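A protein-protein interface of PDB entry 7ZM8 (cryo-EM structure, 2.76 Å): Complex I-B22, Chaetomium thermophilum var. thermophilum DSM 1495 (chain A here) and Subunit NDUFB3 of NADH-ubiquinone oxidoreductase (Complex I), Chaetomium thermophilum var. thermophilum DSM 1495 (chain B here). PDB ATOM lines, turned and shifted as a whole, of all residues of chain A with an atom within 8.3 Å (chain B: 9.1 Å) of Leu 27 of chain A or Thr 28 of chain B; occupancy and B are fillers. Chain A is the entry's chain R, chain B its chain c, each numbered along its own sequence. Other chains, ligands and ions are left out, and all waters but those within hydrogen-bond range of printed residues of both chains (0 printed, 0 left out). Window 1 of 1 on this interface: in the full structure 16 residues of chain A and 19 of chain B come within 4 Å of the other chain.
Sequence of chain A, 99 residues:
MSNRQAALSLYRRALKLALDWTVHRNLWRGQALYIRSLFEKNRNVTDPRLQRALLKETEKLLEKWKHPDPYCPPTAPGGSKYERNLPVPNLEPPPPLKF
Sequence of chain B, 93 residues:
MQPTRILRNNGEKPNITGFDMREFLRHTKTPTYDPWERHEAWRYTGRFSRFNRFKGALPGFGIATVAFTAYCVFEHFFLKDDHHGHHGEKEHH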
ATOM      1  N   ALA A  18      17.606  21.528  -1.014  1.00  0.00           N
ATOM      2  CA  ALA A  18      17.915  20.397  -0.128  1.00  0.00           C
ATOM      3  C   ALA A  18      18.530  20.873   1.199  1.00  0.00           C
ATOM      4  O   ALA A  18      18.153  20.315   2.224  1.00  0.00           O
ATOM      5  CB  ALA A  18      18.804  19.457  -0.879  1.00  0.00           C
ATOM      6  N   LEU A  19      19.480  21.809   1.179  1.00  0.00           N
ATOM      7  CA  LEU A  19      20.167  22.290   2.400  1.00  0.00           C
ATOM      8  C   LEU A  19      19.219  23.175   3.189  1.00  0.00           C
ATOM      9  O   LEU A  19      19.449  23.371   4.387  1.00  0.00           O
ATOM     10  CB  LEU A  19      21.457  23.033   2.039  1.00  0.00           C
ATOM     11  CG  LEU A  19      22.414  23.317   3.194  1.00  0.00           C
ATOM     12  CD1 LEU A  19      22.647  22.077   4.037  1.00  0.00           C
ATOM     13  CD2 LEU A  19      23.727  23.863   2.674  1.00  0.00           C
ATOM     14  N   THR A  22      16.834  20.283   4.748  1.00  0.00           N
ATOM     15  CA  THR A  22      17.708  19.534   5.685  1.00  0.00           C
ATOM     16  C   THR A  22      18.801  20.477   6.175  1.00  0.00           C
ATOM     17  O   THR A  22      19.701  20.785   5.393  1.00  0.00           O
ATOM     18  CB  THR A  22      18.404  18.395   4.945  1.00  0.00           C
ATOM     19  OG1 THR A  22      17.380  17.762   4.185  1.00  0.00           O
ATOM     20  CG2 THR A  22      19.089  17.417   5.868  1.00  0.00           C
ATOM     21  N   VAL A  23      18.716  20.904   7.426  1.00  0.00           N
ATOM     22  CA  VAL A  23      19.643  21.943   7.964  1.00  0.00           C
ATOM     23  C   VAL A  23      21.012  21.336   8.220  1.00  0.00           C
ATOM     24  O   VAL A  23      22.009  22.023   7.985  1.00  0.00           O
ATOM     25  CB  VAL A  23      19.038  22.574   9.230  1.00  0.00           C
ATOM     26  CG1 VAL A  23      20.028  23.420  10.011  1.00  0.00           C
ATOM     27  CG2 VAL A  23      17.759  23.336   8.926  1.00  0.00           C
ATOM     28  N   HIS A  24      21.039  20.059   8.572  1.00  0.00           N
ATOM     29  CA  HIS A  24      22.309  19.336   8.840  1.00  0.00           C
ATOM     30  C   HIS A  24      23.058  19.003   7.547  1.00  0.00           C
ATOM     31  O   HIS A  24      22.506  18.252   6.743  1.00  0.00           O
ATOM     32  CB  HIS A  24      21.938  18.127   9.688  1.00  0.00           C
ATOM     33  CG  HIS A  24      21.167  18.523  10.898  1.00  0.00           C
ATOM     34  ND1 HIS A  24      19.838  18.213  11.059  1.00  0.00           N
ATOM     35  CD2 HIS A  24      21.522  19.251  11.977  1.00  0.00           C
ATOM     36  CE1 HIS A  24      19.411  18.705  12.201  1.00  0.00           C
ATOM     37  NE2 HIS A  24      20.426  19.348  12.783  1.00  0.00           N
ATOM     38  N   ARG A  25      24.303  19.473   7.415  1.00  0.00           N
ATOM     39  CA  ARG A  25      25.105  19.323   6.168  1.00  0.00           C
ATOM     40  C   ARG A  25      25.466  17.877   5.837  1.00  0.00           C
ATOM     41  O   ARG A  25      25.490  17.566   4.654  1.00  0.00           O
ATOM     42  CB  ARG A  25      26.313  20.259   6.219  1.00  0.00           C
ATOM     43  CG  ARG A  25      25.958  21.731   6.357  1.00  0.00           C
ATOM     44  CD  ARG A  25      27.212  22.574   6.358  1.00  0.00           C
ATOM     45  NE  ARG A  25      28.051  22.301   5.201  1.00  0.00           N
ATOM     46  CZ  ARG A  25      27.940  22.906   4.026  1.00  0.00           C
ATOM     47  NH1 ARG A  25      27.014  23.828   3.836  1.00  0.00           N
ATOM     48  NH2 ARG A  25      28.754  22.581   3.039  1.00  0.00           N
ATOM     49  N   ASN A  26      25.799  17.055   6.819  1.00  0.00           N
ATOM     50  CA  ASN A  26      26.046  15.608   6.584  1.00  0.00           C
ATOM     51  C   ASN A  26      24.868  14.979   5.850  1.00  0.00           C
ATOM     52  O   ASN A  26      25.105  14.306   4.856  1.00  0.00           O
ATOM     53  CB  ASN A  26      26.272  14.841   7.891  1.00  0.00           C
ATOM     54  CG  ASN A  26      25.412  15.274   9.058  1.00  0.00           C
ATOM     55  OD1 ASN A  26      24.545  16.128   8.929  1.00  0.00           O
ATOM     56  ND2 ASN A  26      25.647  14.677  10.212  1.00  0.00           N
ATOM     57  N   LEU A  27      23.652  15.155   6.358  1.00  0.00           N
ATOM     58  CA  LEU A  27      22.471  14.535   5.770  1.00  0.00           C
ATOM     59  C   LEU A  27      22.208  15.072   4.369  1.00  0.00           C
ATOM     60  O   LEU A  27      21.863  14.309   3.461  1.00  0.00           O
ATOM     61  CB  LEU A  27      21.253  14.767   6.662  1.00  0.00           C
ATOM     62  CG  LEU A  27      21.001  13.858   7.860  1.00  0.00           C
ATOM     63  CD1 LEU A  27      20.745  12.451   7.398  1.00  0.00           C
ATOM     64  CD2 LEU A  27      22.147  13.892   8.852  1.00  0.00           C
ATOM     65  N   TRP A  28      22.365  16.383   4.179  1.00  0.00           N
ATOM     66  CA  TRP A  28      22.177  16.980   2.862  1.00  0.00           C
ATOM     67  C   TRP A  28      23.219  16.481   1.882  1.00  0.00           C
ATOM     68  O   TRP A  28      22.979  16.459   0.671  1.00  0.00           O
ATOM     69  CB  TRP A  28      22.225  18.501   2.972  1.00  0.00           C
ATOM     70  CG  TRP A  28      22.572  19.224   1.711  1.00  0.00           C
ATOM     71  CD1 TRP A  28      21.735  19.520   0.682  1.00  0.00           C
ATOM     72  CD2 TRP A  28      23.846  19.770   1.359  1.00  0.00           C
ATOM     73  NE1 TRP A  28      22.403  20.207  -0.292  1.00  0.00           N
ATOM     74  CE2 TRP A  28      23.705  20.372   0.100  1.00  0.00           C
ATOM     75  CE3 TRP A  28      25.094  19.803   1.984  1.00  0.00           C
ATOM     76  CZ2 TRP A  28      24.761  20.999  -0.547  1.00  0.00           C
ATOM     77  CZ3 TRP A  28      26.136  20.424   1.342  1.00  0.00           C
ATOM     78  CH2 TRP A  28      25.965  21.016   0.090  1.00  0.00           C
ATOM     79  N   ARG A  29      24.377  16.071   2.388  1.00  0.00           N
ATOM     80  CA  ARG A  29      25.414  15.528   1.524  1.00  0.00           C
ATOM     81  C   ARG A  29      24.929  14.272   0.808  1.00  0.00           C
ATOM     82  O   ARG A  29      25.150  14.110  -0.395  1.00  0.00           O
ATOM     83  CB  ARG A  29      26.661  15.251   2.358  1.00  0.00           C
ATOM     84  CG  ARG A  29      27.916  15.115   1.577  1.00  0.00           C
ATOM     85  CD  ARG A  29      28.369  16.452   1.040  1.00  0.00           C
ATOM     86  NE  ARG A  29      27.845  16.700  -0.295  1.00  0.00           N
ATOM     87  CZ  ARG A  29      28.039  17.821  -0.970  1.00  0.00           C
ATOM     88  NH1 ARG A  29      28.764  18.789  -0.437  1.00  0.00           N
ATOM     89  NH2 ARG A  29      27.517  17.971  -2.177  1.00  0.00           N
ATOM     90  N   GLY A  30      24.249  13.378   1.526  1.00  0.00           N
ATOM     91  CA  GLY A  30      23.666  12.218   0.875  1.00  0.00           C
ATOM     92  C   GLY A  30      22.560  12.590  -0.092  1.00  0.00           C
ATOM     93  O   GLY A  30      22.413  11.976  -1.149  1.00  0.00           O
ATOM     94  N   GLN A  31      21.761  13.598   0.264  1.00  0.00           N
ATOM     95  CA  GLN A  31      20.736  14.095  -0.645  1.00  0.00           C
ATOM     96  C   GLN A  31      21.356  14.709  -1.889  1.00  0.00           C
ATOM     97  O   GLN A  31      20.810  14.586  -2.990  1.00  0.00           O
ATOM     98  CB  GLN A  31      19.861  15.126   0.060  1.00  0.00           C
ATOM     99  CG  GLN A  31      19.139  14.601   1.270  1.00  0.00           C
ATOM    100  CD  GLN A  31      18.283  15.656   1.920  1.00  0.00           C
ATOM    101  OE1 GLN A  31      17.681  15.426   2.966  1.00  0.00           O
ATOM    102  NE2 GLN A  31      18.229  16.827   1.308  1.00  0.00           N
ATOM    103  N   ALA A  32      22.484  15.400  -1.727  1.00  0.00           N
ATOM    104  CA  ALA A  32      23.143  16.046  -2.856  1.00  0.00           C
ATOM    105  C   ALA A  32      23.659  15.034  -3.867  1.00  0.00           C
ATOM    106  O   ALA A  32      23.568  15.274  -5.076  1.00  0.00           O
ATOM    107  CB  ALA A  32      24.278  16.932  -2.353  1.00  0.00           C
ATOM    108  N   LEU A  33      24.209  13.911  -3.404  1.00  0.00           N
ATOM    109  CA  LEU A  33      24.645  12.870  -4.329  1.00  0.00           C
ATOM    110  C   LEU A  33      23.479  12.253  -5.084  1.00  0.00           C
ATOM    111  O   LEU A  33      23.661  11.761  -6.201  1.00  0.00           O
ATOM    112  CB  LEU A  33      25.424  11.781  -3.591  1.00  0.00           C
ATOM    113  CG  LEU A  33      26.899  12.009  -3.244  1.00  0.00           C
ATOM    114  CD1 LEU A  33      27.191  13.352  -2.595  1.00  0.00           C
ATOM    115  CD2 LEU A  33      27.394  10.883  -2.360  1.00  0.00           C
ATOM    116  N   TYR A  34      22.285  12.250  -4.495  1.00  0.00           N
ATOM    117  CA  TYR A  34      21.135  11.670  -5.175  1.00  0.00           C
ATOM    118  C   TYR A  34      20.608  12.609  -6.255  1.00  0.00           C
ATOM    119  O   TYR A  34      20.199  12.157  -7.330  1.00  0.00           O
ATOM    120  CB  TYR A  34      20.055  11.316  -4.149  1.00  0.00           C
ATOM    121  CG  TYR A  34      18.709  10.951  -4.727  1.00  0.00           C
ATOM    122  CD1 TYR A  34      17.765  11.920  -5.031  1.00  0.00           C
ATOM    123  CD2 TYR A  34      18.393   9.633  -4.987  1.00  0.00           C
ATOM    124  CE1 TYR A  34      16.547  11.578  -5.562  1.00  0.00           C
ATOM    125  CE2 TYR A  34      17.181   9.283  -5.521  1.00  0.00           C
ATOM    126  CZ  TYR A  34      16.261  10.257  -5.808  1.00  0.00           C
ATOM    127  OH  TYR A  34      15.045   9.901  -6.343  1.00  0.00           O
ATOM    128  N   PHE B  19      13.168  11.693 -10.227  1.00  0.00           N
ATOM    129  CA  PHE B  19      12.995  12.048  -8.803  1.00  0.00           C
ATOM    130  C   PHE B  19      11.858  11.278  -8.151  1.00  0.00           C
ATOM    131  O   PHE B  19      10.722  11.383  -8.633  1.00  0.00           O
ATOM    132  CB  PHE B  19      12.719  13.538  -8.624  1.00  0.00           C
ATOM    133  CG  PHE B  19      12.782  13.978  -7.184  1.00  0.00           C
ATOM    134  CD1 PHE B  19      14.001  14.197  -6.568  1.00  0.00           C
ATOM    135  CD2 PHE B  19      11.629  14.134  -6.435  1.00  0.00           C
ATOM    136  CE1 PHE B  19      14.065  14.584  -5.240  1.00  0.00           C
ATOM    137  CE2 PHE B  19      11.696  14.515  -5.105  1.00  0.00           C
ATOM    138  CZ  PHE B  19      12.914  14.743  -4.511  1.00  0.00           C
ATOM    139  N   ASP B  20      12.159  10.523  -7.105  1.00  0.00           N
ATOM    140  CA  ASP B  20      11.131   9.899  -6.293  1.00  0.00           C
ATOM    141  C   ASP B  20      11.411  10.322  -4.865  1.00  0.00           C
ATOM    142  O   ASP B  20      12.559  10.256  -4.419  1.00  0.00           O
ATOM    143  CB  ASP B  20      11.152   8.373  -6.428  1.00  0.00           C
ATOM    144  CG  ASP B  20      10.010   7.706  -5.691  1.00  0.00           C
ATOM    145  OD1 ASP B  20       8.862   7.778  -6.177  1.00  0.00           O
ATOM    146  OD2 ASP B  20      10.264   7.106  -4.626  1.00  0.00           O
ATOM    147  N   MET B  21      10.382  10.781  -4.157  1.00  0.00           N
ATOM    148  CA  MET B  21      10.625  11.302  -2.818  1.00  0.00           C
ATOM    149  C   MET B  21      10.912  10.193  -1.820  1.00  0.00           C
ATOM    150  O   MET B  21      11.651  10.416  -0.857  1.00  0.00           O
ATOM    151  CB  MET B  21       9.452  12.176  -2.373  1.00  0.00           C
ATOM    152  CG  MET B  21       9.663  12.853  -1.031  1.00  0.00           C
ATOM    153  SD  MET B  21      11.046  14.013  -1.003  1.00  0.00           S
ATOM    154  CE  MET B  21      10.461  15.383  -1.960  1.00  0.00           C
ATOM    155  N   ARG B  22      10.374   8.995  -2.037  1.00  0.00           N
ATOM    156  CA  ARG B  22      10.731   7.875  -1.174  1.00  0.00           C
ATOM    157  C   ARG B  22      12.215   7.556  -1.292  1.00  0.00           C
ATOM    158  O   ARG B  22      12.895   7.322  -0.286  1.00  0.00           O
ATOM    159  CB  ARG B  22       9.884   6.649  -1.520  1.00  0.00           C
ATOM    160  CG  ARG B  22       8.437   6.750  -1.073  1.00  0.00           C
ATOM    161  CD  ARG B  22       8.333   6.928   0.430  1.00  0.00           C
ATOM    162  NE  ARG B  22       6.966   7.220   0.851  1.00  0.00           N
ATOM    163  CZ  ARG B  22       6.629   7.606   2.077  1.00  0.00           C
ATOM    164  NH1 ARG B  22       7.559   7.757   3.008  1.00  0.00           N
ATOM    165  NH2 ARG B  22       5.358   7.848   2.371  1.00  0.00           N
ATOM    166  N   GLU B  23      12.736   7.546  -2.520  1.00  0.00           N
ATOM    167  CA  GLU B  23      14.159   7.296  -2.722  1.00  0.00           C
ATOM    168  C   GLU B  23      15.001   8.471  -2.252  1.00  0.00           C
ATOM    169  O   GLU B  23      16.140   8.284  -1.814  1.00  0.00           O
ATOM    170  CB  GLU B  23      14.432   7.002  -4.197  1.00  0.00           C
ATOM    171  CG  GLU B  23      13.809   5.712  -4.697  1.00  0.00           C
ATOM    172  CD  GLU B  23      14.449   4.483  -4.087  1.00  0.00           C
ATOM    173  OE1 GLU B  23      15.665   4.518  -3.814  1.00  0.00           O
ATOM    174  OE2 GLU B  23      13.734   3.483  -3.876  1.00  0.00           O
ATOM    175  N   PHE B  24      14.461   9.679  -2.360  1.00  0.00           N
ATOM    176  CA  PHE B  24      15.193  10.873  -1.873  1.00  0.00           C
ATOM    177  C   PHE B  24      15.441  10.717  -0.375  1.00  0.00           C
ATOM    178  O   PHE B  24      16.580  10.936   0.053  1.00  0.00           O
ATOM    179  CB  PHE B  24      14.395  12.135  -2.189  1.00  0.00           C
ATOM    180  CG  PHE B  24      15.004  13.429  -1.718  1.00  0.00           C
ATOM    181  CD1 PHE B  24      16.089  13.984  -2.374  1.00  0.00           C
ATOM    182  CD2 PHE B  24      14.471  14.108  -0.636  1.00  0.00           C
ATOM    183  CE1 PHE B  24      16.633  15.185  -1.951  1.00  0.00           C
ATOM    184  CE2 PHE B  24      15.015  15.307  -0.213  1.00  0.00           C
ATOM    185  CZ  PHE B  24      16.092  15.844  -0.875  1.00  0.00           C
ATOM    186  N   LEU B  25      14.407  10.348   0.388  1.00  0.00           N
ATOM    187  CA  LEU B  25      14.568  10.232   1.833  1.00  0.00           C
ATOM    188  C   LEU B  25      15.440   9.048   2.215  1.00  0.00           C
ATOM    189  O   LEU B  25      16.050   9.057   3.288  1.00  0.00           O
ATOM    190  CB  LEU B  25      13.213  10.120   2.526  1.00  0.00           C
ATOM    191  CG  LEU B  25      12.469  11.414   2.858  1.00  0.00           C
ATOM    192  CD1 LEU B  25      13.238  12.209   3.894  1.00  0.00           C
ATOM    193  CD2 LEU B  25      12.217  12.248   1.643  1.00  0.00           C
ATOM    194  N   ARG B  26      15.493   8.018   1.370  1.00  0.00           N
ATOM    195  CA  ARG B  26      16.353   6.880   1.658  1.00  0.00           C
ATOM    196  C   ARG B  26      17.814   7.288   1.680  1.00  0.00           C
ATOM    197  O   ARG B  26      18.602   6.750   2.464  1.00  0.00           O
ATOM    198  CB  ARG B  26      16.127   5.779   0.627  1.00  0.00           C
ATOM    199  N   HIS B  27      18.190   8.240   0.840  1.00  0.00           N
ATOM    200  CA  HIS B  27      19.560   8.712   0.762  1.00  0.00           C
ATOM    201  C   HIS B  27      19.865   9.811   1.763  1.00  0.00           C
ATOM    202  O   HIS B  27      20.994  10.307   1.788  1.00  0.00           O
ATOM    203  CB  HIS B  27      19.865   9.209  -0.651  1.00  0.00           C
ATOM    204  CG  HIS B  27      20.007   8.113  -1.657  1.00  0.00           C
ATOM    205  ND1 HIS B  27      20.811   8.224  -2.770  1.00  0.00           N
ATOM    206  CD2 HIS B  27      19.444   6.884  -1.722  1.00  0.00           C
ATOM    207  CE1 HIS B  27      20.740   7.111  -3.475  1.00  0.00           C
ATOM    208  NE2 HIS B  27      19.916   6.280  -2.862  1.00  0.00           N
ATOM    209  N   THR B  28      18.896  10.209   2.588  1.00  0.00           N
ATOM    210  CA  THR B  28      19.149  11.184   3.646  1.00  0.00           C
ATOM    211  C   THR B  28      19.934  10.481   4.743  1.00  0.00           C
ATOM    212  O   THR B  28      19.404  10.076   5.779  1.00  0.00           O
ATOM    213  CB  THR B  28      17.855  11.772   4.183  1.00  0.00           C
ATOM    214  OG1 THR B  28      17.097  10.739   4.821  1.00  0.00           O
ATOM    215  CG2 THR B  28      17.044  12.374   3.062  1.00  0.00           C
ATOM    216  N   LYS B  29      21.227  10.336   4.495  1.00  0.00           N
ATOM    217  CA  LYS B  29      22.136   9.673   5.409  1.00  0.00           C
ATOM    218  C   LYS B  29      23.515  10.277   5.201  1.00  0.00           C
ATOM    219  O   LYS B  29      23.684  11.233   4.442  1.00  0.00           O
ATOM    220  CB  LYS B  29      22.133   8.160   5.182  1.00  0.00           C
ATOM    221  N   THR B  30      24.500   9.729   5.891  1.00  0.00           N
ATOM    222  CA  THR B  30      25.880  10.086   5.615  1.00  0.00           C
ATOM    223  C   THR B  30      26.415   9.154   4.539  1.00  0.00           C
ATOM    224  O   THR B  30      26.547   7.951   4.789  1.00  0.00           O
ATOM    225  CB  THR B  30      26.729   9.989   6.873  1.00  0.00           C
ATOM    226  OG1 THR B  30      26.224  10.899   7.858  1.00  0.00           O
ATOM    227  CG2 THR B  30      28.174  10.336   6.566  1.00  0.00           C
ATOM    228  N   PRO B  31      26.717   9.649   3.344  1.00  0.00           N
ATOM    229  CA  PRO B  31      27.091   8.750   2.249  1.00  0.00           C
ATOM    230  C   PRO B  31      28.403   8.035   2.521  1.00  0.00           C
ATOM    231  O   PRO B  31      29.287   8.546   3.212  1.00  0.00           O
ATOM    232  CB  PRO B  31      27.203   9.687   1.041  1.00  0.00           C
ATOM    233  CG  PRO B  31      27.400  11.044   1.617  1.00  0.00           C
ATOM    234  CD  PRO B  31      26.680  11.059   2.925  1.00  0.00           C
ATOM    235  N   TYR B  44      33.180  17.525  12.016  1.00  0.00           N
ATOM    236  CA  TYR B  44      32.753  16.378  12.855  1.00  0.00           C
ATOM    237  C   TYR B  44      33.933  15.881  13.685  1.00  0.00           C
ATOM    238  O   TYR B  44      33.823  14.805  14.291  1.00  0.00           O
ATOM    239  CB  TYR B  44      32.116  15.307  11.974  1.00  0.00           C
ATOM    240  CG  TYR B  44      31.200  15.841  10.906  1.00  0.00           C
ATOM    241  CD1 TYR B  44      29.916  16.259  11.209  1.00  0.00           C
ATOM    242  CD2 TYR B  44      31.622  15.938   9.591  1.00  0.00           C
ATOM    243  CE1 TYR B  44      29.073  16.760  10.234  1.00  0.00           C
ATOM    244  CE2 TYR B  44      30.790  16.432   8.603  1.00  0.00           C
ATOM    245  CZ  TYR B  44      29.510  16.844   8.927  1.00  0.00           C
ATOM    246  OH  TYR B  44      28.690  17.331   7.952  1.00  0.00           O
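The backbone NH of Asn 26 of chain A lies within hydrogen-bond range of the side-chain hydroxyl of Tyr 44 of chain B, 3.1 Å away.
The side-chain hydroxyl (OH) of Tyr 34 of chain A is in hydrogen-bond range of the backbone NH (N) of Asp 20 of chain B, 3.0 Å away.
The backbone carbonyl oxygen (O) of Asn 26 of chain A sits close to the backbone carbonyl oxygen (O) of Lys 29 of chain B, at 3.4 Å.
The side-chain carboxylate (OD2) of Asp 20 of chain B is in hydrogen-bond range of the backbone NH (N) of Glu 23 of chain B, 3.3 Å away.
OE1 of Gln 31 of chain A sits at hydrogen-bond distance from OG1 of Thr 22 of chain A.
The backbone carbonyl oxygen (O) of Leu 25 of chain B lies within hydrogen-bond range of the side-chain hydroxyl (OG1) of Thr 28 of chain B.
OD2 of Asp 20 of chain B sits close to N of Arg 22 of chain B, at 3.2 Å.
Among the printed residues, pairs that only touch across the chains: Arg 25 of chain A with Tyr 44 of chain B (3.9 Å), Asn 26 of chain A with Thr 30 of chain B (3.9 Å), Leu 27 of chain A with Thr 28 of chain B (3.2 Å), Leu 27 of chain A with Lys 29 of chain B (3.6 Å), Gly 30 of chain A with His 27 of chain B (3.3 Å), Gly 30 of chain A with Lys 29 of chain B (3.7 Å), Gly 30 of chain A with Pro 31 of chain B (3.6 Å), Gln 31 of chain A with Phe 24 of chain B (3.2 Å), Gln 31 of chain A with His 27 of chain B (3.7 Å), Gln 31 of chain A with Thr 28 of chain B (3.1 Å), Leu 33 of chain A with Pro 31 of chain B (3.6 Å), Tyr 34 of chain A with Phe 19 of chain B (3.8 Å), Tyr 34 of chain A with Glu 23 of chain B (3.7 Å), Tyr 34 of chain A with Phe 24 of chain B (3.8 Å) and Tyr 34 of chain A with His 27 of chain B (3.5 Å).
Of chain B, only Thr 28 and Lys 29 come within 4 Å of Leu 27 of chain A.
Thr 28 of chain B touches just these residues of chain A: Leu 27 and Gln 31.
Of chain B, only Lys 29, Thr 30 and Tyr 44 come within 4 Å of Asn 26 of chain A.
Lys 29 of chain B touches just these residues of chain A: Asn 26 (3.4 Å), Leu 27 (3.6 Å) and Gly 30 (3.7 Å).
Printed residues of chain A within 4 Å of His 27 of chain B: Gly 30, Gln 31 and Tyr 34.
Printed residues of chain A within 4 Å of Pro 31 of chain B: Gly 30 and Leu 33.
Ala 18 of chain A touches none of the printed residues of chain B.
The nearest residue of chain B that does not touch Leu 27 of chain A is His 27 of chain B (4.4 Å).
The nearest printed residue of chain B that does not touch Gly 30 of chain A is Thr 28 of chain B (5.1 Å).
Printed residues of chain B that touch a printed residue of chain A: Phe 19, Asp 20, Glu 23, Phe 24, His 27, Thr 28, Lys 29, Thr 30, Pro 31 and Tyr 44.
Hydrophobic or aromatic side chains of chain B within 4 Å of the printed part of chain A: Phe 19, Phe 24, His 27, Pro 31 and Tyr 44.
Of the 15 printed residues of chain A, 7 touch a printed residue of chain B.
Hydrophobic or aromatic side chains of chain A that line the printed part of chain B: Leu 27, Leu 33 and Tyr 34.
Along chain A the printed residues that touch a printed residue of chain B span positions 25 to 34.
Among the printed residues, no Asp or Glu carboxylate lies within 4 Å of a Lys or Arg side-chain nitrogen of the other chain.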
